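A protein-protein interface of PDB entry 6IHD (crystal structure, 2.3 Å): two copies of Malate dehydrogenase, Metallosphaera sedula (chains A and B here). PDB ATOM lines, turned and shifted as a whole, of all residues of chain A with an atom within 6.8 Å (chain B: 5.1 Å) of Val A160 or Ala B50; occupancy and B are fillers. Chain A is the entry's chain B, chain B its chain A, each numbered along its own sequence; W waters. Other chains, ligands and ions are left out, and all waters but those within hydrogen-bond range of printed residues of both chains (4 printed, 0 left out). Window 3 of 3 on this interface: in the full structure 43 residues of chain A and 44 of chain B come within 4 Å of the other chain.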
ATOM      1  N   THR A 145      12.837   5.223  23.051  1.00  0.00           N
ATOM      2  CA  THR A 145      14.125   5.872  23.220  1.00  0.00           C
ATOM      3  C   THR A 145      14.729   6.257  21.855  1.00  0.00           C
ATOM      4  O   THR A 145      15.212   7.379  21.660  1.00  0.00           O
ATOM      5  CB  THR A 145      15.115   4.970  24.005  1.00  0.00           C
ATOM      6  OG1 THR A 145      14.715   4.896  25.364  1.00  0.00           O
ATOM      7  CG2 THR A 145      16.604   5.565  23.962  1.00  0.00           C
ATOM      8  N   MET A 146      14.731   5.317  20.918  1.00  0.00           N
ATOM      9  CA  MET A 146      15.356   5.616  19.623  1.00  0.00           C
ATOM     10  C   MET A 146      14.539   6.601  18.774  1.00  0.00           C
ATOM     11  O   MET A 146      15.105   7.369  17.979  1.00  0.00           O
ATOM     12  CB  MET A 146      15.642   4.301  18.887  1.00  0.00           C
ATOM     13  CG  MET A 146      16.644   3.407  19.614  1.00  0.00           C
ATOM     14  SD  MET A 146      18.208   4.299  19.807  1.00  0.00           S
ATOM     15  CE  MET A 146      19.037   3.308  21.015  1.00  0.00           C
ATOM     16  N   ARG A 147      13.218   6.590  18.974  1.00  0.00           N
ATOM     17  CA  ARG A 147      12.320   7.561  18.364  1.00  0.00           C
ATOM     18  C   ARG A 147      12.564   8.961  18.857  1.00  0.00           C
ATOM     19  O   ARG A 147      12.613   9.913  18.090  1.00  0.00           O
ATOM     20  CB  ARG A 147      10.857   7.195  18.611  1.00  0.00           C
ATOM     21  CG  ARG A 147      10.423   6.029  17.767  1.00  0.00           C
ATOM     22  CD  ARG A 147       9.047   5.550  18.170  1.00  0.00           C
ATOM     23  NE  ARG A 147       8.739   4.440  17.294  1.00  0.00           N
ATOM     24  CZ  ARG A 147       7.879   3.465  17.561  1.00  0.00           C
ATOM     25  NH1 ARG A 147       7.213   3.425  18.726  1.00  0.00           N
ATOM     26  NH2 ARG A 147       7.715   2.518  16.650  1.00  0.00           N
ATOM     27  N   ARG A 149      15.373  10.050  20.010  1.00  0.00           N
ATOM     28  CA  ARG A 149      16.697  10.462  19.602  1.00  0.00           C
ATOM     29  C   ARG A 149      16.705  10.934  18.163  1.00  0.00           C
ATOM     30  O   ARG A 149      17.242  11.980  17.874  1.00  0.00           O
ATOM     31  CB  ARG A 149      17.720   9.352  19.891  1.00  0.00           C
ATOM     32  CG  ARG A 149      18.212   9.499  21.331  1.00  0.00           C
ATOM     33  CD  ARG A 149      18.539   8.254  22.157  1.00  0.00           C
ATOM     34  NE  ARG A 149      19.864   7.873  21.861  1.00  0.00           N
ATOM     35  CZ  ARG A 149      20.684   7.137  22.595  1.00  0.00           C
ATOM     36  NH1 ARG A 149      20.400   6.598  23.783  1.00  0.00           N
ATOM     37  NH2 ARG A 149      21.868   6.970  22.049  1.00  0.00           N
ATOM     38  N   SER A 150      16.039  10.203  17.291  1.00  0.00           N
ATOM     39  CA  SER A 150      16.009  10.541  15.883  1.00  0.00           C
ATOM     40  C   SER A 150      15.212  11.813  15.623  1.00  0.00           C
ATOM     41  O   SER A 150      15.537  12.512  14.694  1.00  0.00           O
ATOM     42  CB  SER A 150      15.382   9.408  15.085  1.00  0.00           C
ATOM     43  OG  SER A 150      14.118   9.109  15.653  1.00  0.00           O
ATOM     44  N   PHE A 151      14.169  12.067  16.439  1.00  0.00           N
ATOM     45  CA  PHE A 151      13.352  13.245  16.299  1.00  0.00           C
ATOM     46  C   PHE A 151      14.147  14.486  16.668  1.00  0.00           C
ATOM     47  O   PHE A 151      14.224  15.430  15.922  1.00  0.00           O
ATOM     48  CB  PHE A 151      12.059  13.125  17.135  1.00  0.00           C
ATOM     49  CG  PHE A 151      11.150  14.343  17.041  1.00  0.00           C
ATOM     50  CD1 PHE A 151      10.282  14.489  15.990  1.00  0.00           C
ATOM     51  CD2 PHE A 151      11.190  15.339  18.015  1.00  0.00           C
ATOM     52  CE1 PHE A 151       9.486  15.621  15.870  1.00  0.00           C
ATOM     53  CE2 PHE A 151      10.405  16.474  17.911  1.00  0.00           C
ATOM     54  CZ  PHE A 151       9.547  16.618  16.839  1.00  0.00           C
ATOM     55  N   ALA A 153      17.302  14.729  16.616  1.00  0.00           N
ATOM     56  CA  ALA A 153      18.315  14.863  15.567  1.00  0.00           C
ATOM     57  C   ALA A 153      17.773  15.606  14.345  1.00  0.00           C
ATOM     58  O   ALA A 153      18.401  16.546  13.929  1.00  0.00           O
ATOM     59  CB  ALA A 153      18.911  13.500  15.192  1.00  0.00           C
ATOM     60  N   LYS A 154      16.625  15.199  13.792  1.00  0.00           N
ATOM     61  CA  LYS A 154      16.061  15.804  12.549  1.00  0.00           C
ATOM     62  C   LYS A 154      15.680  17.268  12.792  1.00  0.00           C
ATOM     63  O   LYS A 154      15.966  18.129  11.974  1.00  0.00           O
ATOM     64  CB  LYS A 154      14.844  15.022  12.019  1.00  0.00           C
ATOM     65  CG  LYS A 154      14.459  15.328  10.589  1.00  0.00           C
ATOM     66  CD  LYS A 154      13.588  14.262   9.920  1.00  0.00           C
ATOM     67  CE  LYS A 154      12.081  14.499  10.092  1.00  0.00           C
ATOM     68  NZ  LYS A 154      11.227  13.433   9.481  1.00  0.00           N
ATOM     69  N   ILE A 158      21.121  17.739  13.113  1.00  0.00           N
ATOM     70  CA  ILE A 158      22.387  17.117  13.527  1.00  0.00           C
ATOM     71  C   ILE A 158      22.318  15.619  13.344  1.00  0.00           C
ATOM     72  O   ILE A 158      21.250  15.070  13.208  1.00  0.00           O
ATOM     73  CB  ILE A 158      22.730  17.422  14.975  1.00  0.00           C
ATOM     74  CG1 ILE A 158      21.669  16.858  15.930  1.00  0.00           C
ATOM     75  CG2 ILE A 158      22.868  18.933  15.148  1.00  0.00           C
ATOM     76  CD1 ILE A 158      21.948  17.210  17.366  1.00  0.00           C
ATOM     77  N   PRO A 159      23.471  14.946  13.327  1.00  0.00           N
ATOM     78  CA  PRO A 159      23.370  13.506  13.259  1.00  0.00           C
ATOM     79  C   PRO A 159      22.838  12.928  14.563  1.00  0.00           C
ATOM     80  O   PRO A 159      23.068  13.504  15.651  1.00  0.00           O
ATOM     81  CB  PRO A 159      24.792  13.073  13.032  1.00  0.00           C
ATOM     82  CG  PRO A 159      25.580  14.136  13.668  1.00  0.00           C
ATOM     83  CD  PRO A 159      24.871  15.366  13.201  1.00  0.00           C
ATOM     84  N   VAL A 160      22.169  11.769  14.438  1.00  0.00           N
ATOM     85  CA  VAL A 160      21.590  11.075  15.590  1.00  0.00           C
ATOM     86  C   VAL A 160      22.646  10.619  16.601  1.00  0.00           C
ATOM     87  O   VAL A 160      22.395  10.488  17.820  1.00  0.00           O
ATOM     88  CB  VAL A 160      20.684   9.903  15.147  1.00  0.00           C
ATOM     89  CG1 VAL A 160      21.489   8.761  14.530  1.00  0.00           C
ATOM     90  CG2 VAL A 160      19.850   9.436  16.329  1.00  0.00           C
ATOM     91  N   THR A 161      23.857  10.431  16.078  1.00  0.00           N
ATOM     92  CA  THR A 161      24.981  10.044  16.887  1.00  0.00           C
ATOM     93  C   THR A 161      25.387  11.172  17.913  1.00  0.00           C
ATOM     94  O   THR A 161      26.074  10.895  18.896  1.00  0.00           O
ATOM     95  CB  THR A 161      26.133   9.616  15.970  1.00  0.00           C
ATOM     96  OG1 THR A 161      26.442  10.657  15.051  1.00  0.00           O
ATOM     97  CG2 THR A 161      25.758   8.275  15.135  1.00  0.00           C
ATOM     98  N   SER A 162      24.922  12.396  17.711  1.00  0.00           N
ATOM     99  CA  SER A 162      25.145  13.478  18.666  1.00  0.00           C
ATOM    100  C   SER A 162      24.040  13.599  19.707  1.00  0.00           C
ATOM    101  O   SER A 162      24.101  14.461  20.525  1.00  0.00           O
ATOM    102  CB  SER A 162      25.338  14.802  17.936  1.00  0.00           C
ATOM    103  OG  SER A 162      26.564  14.765  17.231  1.00  0.00           O
ATOM    104  N   VAL A 163      23.086  12.682  19.739  1.00  0.00           N
ATOM    105  CA  VAL A 163      22.044  12.744  20.732  1.00  0.00           C
ATOM    106  C   VAL A 163      22.140  11.501  21.638  1.00  0.00           C
ATOM    107  O   VAL A 163      22.194  10.317  21.176  1.00  0.00           O
ATOM    108  CB  VAL A 163      20.672  12.843  20.036  1.00  0.00           C
ATOM    109  CG1 VAL A 163      19.561  13.021  21.041  1.00  0.00           C
ATOM    110  CG2 VAL A 163      20.627  14.017  19.031  1.00  0.00           C
ATOM    111  N   ASP A 164      22.128  11.775  22.927  1.00  0.00           N
ATOM    112  CA  ASP A 164      22.077  10.753  23.942  1.00  0.00           C
ATOM    113  C   ASP A 164      20.787  10.856  24.773  1.00  0.00           C
ATOM    114  O   ASP A 164      20.221  11.941  24.917  1.00  0.00           O
ATOM    115  CB  ASP A 164      23.324  10.883  24.838  1.00  0.00           C
ATOM    116  CG  ASP A 164      23.883   9.508  25.301  1.00  0.00           C
ATOM    117  OD1 ASP A 164      23.065   8.538  25.424  1.00  0.00           O
ATOM    118  OD2 ASP A 164      25.131   9.417  25.527  1.00  0.00           O
ATOM    119  N   ILE A 224      15.627  -2.362  16.393  1.00  0.00           N
ATOM    120  CA  ILE A 224      15.933  -1.921  17.756  1.00  0.00           C
ATOM    121  C   ILE A 224      15.909  -3.120  18.732  1.00  0.00           C
ATOM    122  O   ILE A 224      16.800  -3.231  19.589  1.00  0.00           O
ATOM    123  CB  ILE A 224      14.986  -0.805  18.197  1.00  0.00           C
ATOM    124  CG1 ILE A 224      15.264   0.448  17.368  1.00  0.00           C
ATOM    125  CG2 ILE A 224      15.129  -0.514  19.687  1.00  0.00           C
ATOM    126  CD1 ILE A 224      14.055   1.353  17.148  1.00  0.00           C
ATOM    127  N   ASP A 227      18.820  -5.303  18.217  1.00  0.00           N
ATOM    128  CA  ASP A 227      20.027  -4.776  18.877  1.00  0.00           C
ATOM    129  C   ASP A 227      20.049  -5.133  20.379  1.00  0.00           C
ATOM    130  O   ASP A 227      21.124  -5.198  21.009  1.00  0.00           O
ATOM    131  CB  ASP A 227      20.117  -3.274  18.742  1.00  0.00           C
ATOM    132  CG  ASP A 227      21.119  -2.809  17.652  1.00  0.00           C
ATOM    133  OD1 ASP A 227      21.598  -3.558  16.775  1.00  0.00           O
ATOM    134  OD2 ASP A 227      21.456  -1.622  17.699  1.00  0.00           O
ATOM    135  N   ARG A 238      25.457  -2.602  26.684  1.00  0.00           N
ATOM    136  CA  ARG A 238      24.708  -1.405  26.279  1.00  0.00           C
ATOM    137  C   ARG A 238      23.649  -1.150  27.292  1.00  0.00           C
ATOM    138  O   ARG A 238      22.964  -2.039  27.692  1.00  0.00           O
ATOM    139  CB  ARG A 238      24.064  -1.583  24.932  1.00  0.00           C
ATOM    140  CG  ARG A 238      25.105  -1.733  23.873  1.00  0.00           C
ATOM    141  CD  ARG A 238      24.479  -1.664  22.521  1.00  0.00           C
ATOM    142  NE  ARG A 238      23.861  -0.383  22.182  1.00  0.00           N
ATOM    143  CZ  ARG A 238      23.254  -0.153  21.011  1.00  0.00           C
ATOM    144  NH1 ARG A 238      23.131  -1.126  20.077  1.00  0.00           N
ATOM    145  NH2 ARG A 238      22.808   1.059  20.738  1.00  0.00           N
ATOM    146  N   LEU B  45      12.789   3.995   9.136  1.00  0.00           N
ATOM    147  CA  LEU B  45      14.238   3.952   8.868  1.00  0.00           C
ATOM    148  C   LEU B  45      14.997   4.754   9.870  1.00  0.00           C
ATOM    149  O   LEU B  45      15.967   4.244  10.382  1.00  0.00           O
ATOM    150  CB  LEU B  45      14.620   4.410   7.455  1.00  0.00           C
ATOM    151  CG  LEU B  45      14.085   3.470   6.329  1.00  0.00           C
ATOM    152  CD1 LEU B  45      14.246   4.080   4.944  1.00  0.00           C
ATOM    153  CD2 LEU B  45      14.756   2.117   6.389  1.00  0.00           C
ATOM    154  N   ARG B  46      14.525   5.969  10.196  1.00  0.00           N
ATOM    155  CA  ARG B  46      15.204   6.851  11.142  1.00  0.00           C
ATOM    156  C   ARG B  46      15.272   6.258  12.545  1.00  0.00           C
ATOM    157  O   ARG B  46      16.295   6.408  13.213  1.00  0.00           O
ATOM    158  CB  ARG B  46      14.555   8.242  11.197  1.00  0.00           C
ATOM    159  CG  ARG B  46      15.037   9.154  10.084  1.00  0.00           C
ATOM    160  CD  ARG B  46      14.233  10.437   9.908  1.00  0.00           C
ATOM    161  NE  ARG B  46      14.661  11.039   8.644  1.00  0.00           N
ATOM    162  CZ  ARG B  46      15.811  11.708   8.452  1.00  0.00           C
ATOM    163  NH1 ARG B  46      16.683  11.973   9.458  1.00  0.00           N
ATOM    164  NH2 ARG B  46      16.088  12.135   7.225  1.00  0.00           N
ATOM    165  N   HIS B  47      14.216   5.537  12.946  1.00  0.00           N
ATOM    166  CA  HIS B  47      14.240   4.894  14.239  1.00  0.00           C
ATOM    167  C   HIS B  47      15.234   3.716  14.281  1.00  0.00           C
ATOM    168  O   HIS B  47      15.995   3.557  15.253  1.00  0.00           O
ATOM    169  CB  HIS B  47      12.841   4.404  14.647  1.00  0.00           C
ATOM    170  CG  HIS B  47      11.797   5.438  14.547  1.00  0.00           C
ATOM    171  ND1 HIS B  47      10.481   5.131  14.343  1.00  0.00           N
ATOM    172  CD2 HIS B  47      11.875   6.786  14.570  1.00  0.00           C
ATOM    173  CE1 HIS B  47       9.777   6.241  14.261  1.00  0.00           C
ATOM    174  NE2 HIS B  47      10.606   7.263  14.381  1.00  0.00           N
ATOM    175  N   ALA B  48      15.217   2.894  13.242  1.00  0.00           N
ATOM    176  CA  ALA B  48      16.244   1.881  13.077  1.00  0.00           C
ATOM    177  C   ALA B  48      17.654   2.477  13.029  1.00  0.00           C
ATOM    178  O   ALA B  48      18.568   1.956  13.663  1.00  0.00           O
ATOM    179  CB  ALA B  48      16.018   1.069  11.821  1.00  0.00           C
ATOM    180  N   PHE B  49      17.831   3.582  12.324  1.00  0.00           N
ATOM    181  CA  PHE B  49      19.165   4.169  12.243  1.00  0.00           C
ATOM    182  C   PHE B  49      19.714   4.572  13.580  1.00  0.00           C
ATOM    183  O   PHE B  49      20.923   4.547  13.775  1.00  0.00           O
ATOM    184  CB  PHE B  49      19.179   5.427  11.386  1.00  0.00           C
ATOM    185  CG  PHE B  49      18.978   5.202   9.938  1.00  0.00           C
ATOM    186  CD1 PHE B  49      18.917   3.915   9.379  1.00  0.00           C
ATOM    187  CD2 PHE B  49      18.889   6.310   9.096  1.00  0.00           C
ATOM    188  CE1 PHE B  49      18.736   3.765   8.026  1.00  0.00           C
ATOM    189  CE2 PHE B  49      18.717   6.160   7.719  1.00  0.00           C
ATOM    190  CZ  PHE B  49      18.630   4.879   7.182  1.00  0.00           C
ATOM    191  N   ALA B  50      18.849   4.993  14.485  1.00  0.00           N
ATOM    192  CA  ALA B  50      19.343   5.599  15.738  1.00  0.00           C
ATOM    193  C   ALA B  50      20.141   4.600  16.593  1.00  0.00           C
ATOM    194  O   ALA B  50      21.180   4.957  17.163  1.00  0.00           O
ATOM    195  CB  ALA B  50      18.184   6.164  16.554  1.00  0.00           C
ATOM    196  N   THR B  51      19.638   3.372  16.665  1.00  0.00           N
ATOM    197  CA  THR B  51      20.273   2.279  17.366  1.00  0.00           C
ATOM    198  C   THR B  51      21.587   1.791  16.766  1.00  0.00           C
ATOM    199  O   THR B  51      22.374   1.213  17.493  1.00  0.00           O
ATOM    200  CB  THR B  51      19.307   1.053  17.512  1.00  0.00           C
ATOM    201  OG1 THR B  51      19.858   0.116  18.425  1.00  0.00           O
ATOM    202  CG2 THR B  51      19.140   0.353  16.252  1.00  0.00           C
ATOM    203  N   LYS B  52      21.775   1.919  15.453  1.00  0.00           N
ATOM    204  CA  LYS B  52      23.009   1.504  14.766  1.00  0.00           C
ATOM    205  C   LYS B  52      24.007   2.648  14.588  1.00  0.00           C
ATOM    206  O   LYS B  52      25.129   2.389  14.173  1.00  0.00           O
ATOM    207  CB  LYS B  52      22.738   0.970  13.351  1.00  0.00           C
ATOM    208  CG  LYS B  52      21.864  -0.281  13.193  1.00  0.00           C
ATOM    209  CD  LYS B  52      22.460  -1.535  13.825  1.00  0.00           C
ATOM    210  CE  LYS B  52      21.889  -2.798  13.189  1.00  0.00           C
ATOM    211  NZ  LYS B  52      21.842  -3.893  14.195  1.00  0.00           N
ATOM    212  N   GLY B  53      23.627   3.902  14.843  1.00  0.00           N
ATOM    213  CA  GLY B  53      24.532   5.060  14.542  1.00  0.00           C
ATOM    214  C   GLY B  53      24.648   5.410  13.084  1.00  0.00           C
ATOM    215  O   GLY B  53      25.588   6.108  12.656  1.00  0.00           O
ATOM    216  N   ILE B  54      23.655   4.968  12.303  1.00  0.00           N
ATOM    217  CA  ILE B  54      23.627   5.252  10.907  1.00  0.00           C
ATOM    218  C   ILE B  54      23.140   6.709  10.709  1.00  0.00           C
ATOM    219  O   ILE B  54      22.112   7.107  11.260  1.00  0.00           O
ATOM    220  CB  ILE B  54      22.690   4.290  10.172  1.00  0.00           C
ATOM    221  CG1 ILE B  54      23.286   2.901  10.196  1.00  0.00           C
ATOM    222  CG2 ILE B  54      22.464   4.789   8.755  1.00  0.00           C
ATOM    223  CD1 ILE B  54      22.369   1.844   9.633  1.00  0.00           C
HETATM  224  O   HOH W   1      24.129  -1.547  16.566  1.00  0.00           O
HETATM  225  O   HOH W   2      16.750  11.165  12.262  1.00  0.00           O
HETATM  226  O   HOH W   3      18.269  -0.829  20.778  1.00  0.00           O
HETATM  227  O   HOH W   4       9.204   2.713  14.281  1.00  0.00           O
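Water W4 bridges ND1 of His B47 (2.7 Å) and NH2 of Arg A147 (2.8 Å).
Water W1 lies within hydrogen-bond range of the side-chain carboxylate of Asp A227 and the backbone carbonyl oxygen of Thr B51.
Water W2 bridges the guanidinium group (NH1) of Arg B46 and the backbone carbonyl oxygen (O) of Ser A150.
Water W3 lies within hydrogen-bond range of the side-chain hydroxyl of Thr B51 and the backbone carbonyl oxygen of Ile A224.
Of the 10 printed residues of chain B, 7 touch a printed residue of chain A.
Hydrophobic or aromatic side chains of chain B that line the printed part of chain A: His B47 and Ala B50.
Of the 18 printed residues of chain A, 9 touch a printed residue of chain B.
Hydrophobic or aromatic side chains of chain A that line the printed part of chain B: Met A146, Val A160 and Ile A224.
Along chain A the printed residues that touch a printed residue of chain B span positions 146 to 238.
Among the printed residues, Asp or Glu carboxylates within 4 Å of a Lys or Arg side-chain nitrogen of the other chain: Asp A227 with Lys B52.
The backbone carbonyl oxygen (O) of Phe B49 lies within hydrogen-bond range of the backbone NH (N) of Ile B54.
The backbone carbonyl oxygen of Met A146 is in hydrogen-bond range of the side-chain hydroxyl of Ser A150 (3.1 Å).
The backbone carbonyl oxygen (O) of Arg A147 lies within hydrogen-bond range of the side-chain hydroxyl (OG) of Ser A150.
The side-chain carboxylate (OD2) of Asp A227 lies within salt-bridge range of the guanidinium group (NH1) of Arg A238, at 3.0 Å.
No position is printed for both chains.
Of the 14 pairs that touch across the chains among the printed residues, none has its exchanged pair printed and touching as well.
ND1 of His B47 sits at hydrogen-bond distance from NE of Arg A147.
N of Thr B51 is in hydrogen-bond range of SD of Met A146.
The side-chain hydroxyl of Thr B51 lies within hydrogen-bond range of the side-chain carboxylate of Asp A227, at 2.5 Å.
The backbone carbonyl oxygen (O) of Thr B51 is in hydrogen-bond range of the guanidinium group (NH2) of Arg A238, at 3.3 Å.
The side-chain carboxylate of Asp A227 is in salt-bridge range of the side-chain amino group of Lys B52, at 2.6 Å.
Of the printed residues of chain B, Val A160 touches Ala B50 (3.7 Å) and Ile B54 (3.7 Å).
Of chain A, only Met A146 (3.6 Å) and Val A160 (3.7 Å) come within 4 Å of Ala B50.
Printed residues of chain B within 4 Å of Asp A227: Thr B51 and Lys B52.
Of the printed residues of chain B, Met A146 touches His B47, Ala B50 and Thr B51.
The nearest residue of chain B that does not touch Val A160 is Phe B49 (4.3 Å).
Met A146 touches His B47 (CB to O, 3.7 Å).
Met A146 touches Ala B50 (O to CB, 3.6 Å).
CB of Ser A150 touches O of Arg B46 (3.7 Å).
Ser A150 touches His B47 (OG to CD2, 3.4 Å).
Arg B46 touches Lys A154 (NE to CD, 3.6 Å).
Val A160 touches Ala B50 (CG2 to CB, 3.7 Å).
Ile B54 touches Val A160.
CG2 of Thr A161 touches O of Gly B53, at 3.3 Å.
CD1 of Ile A224 touches O of His B47, 3.5 Å away.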
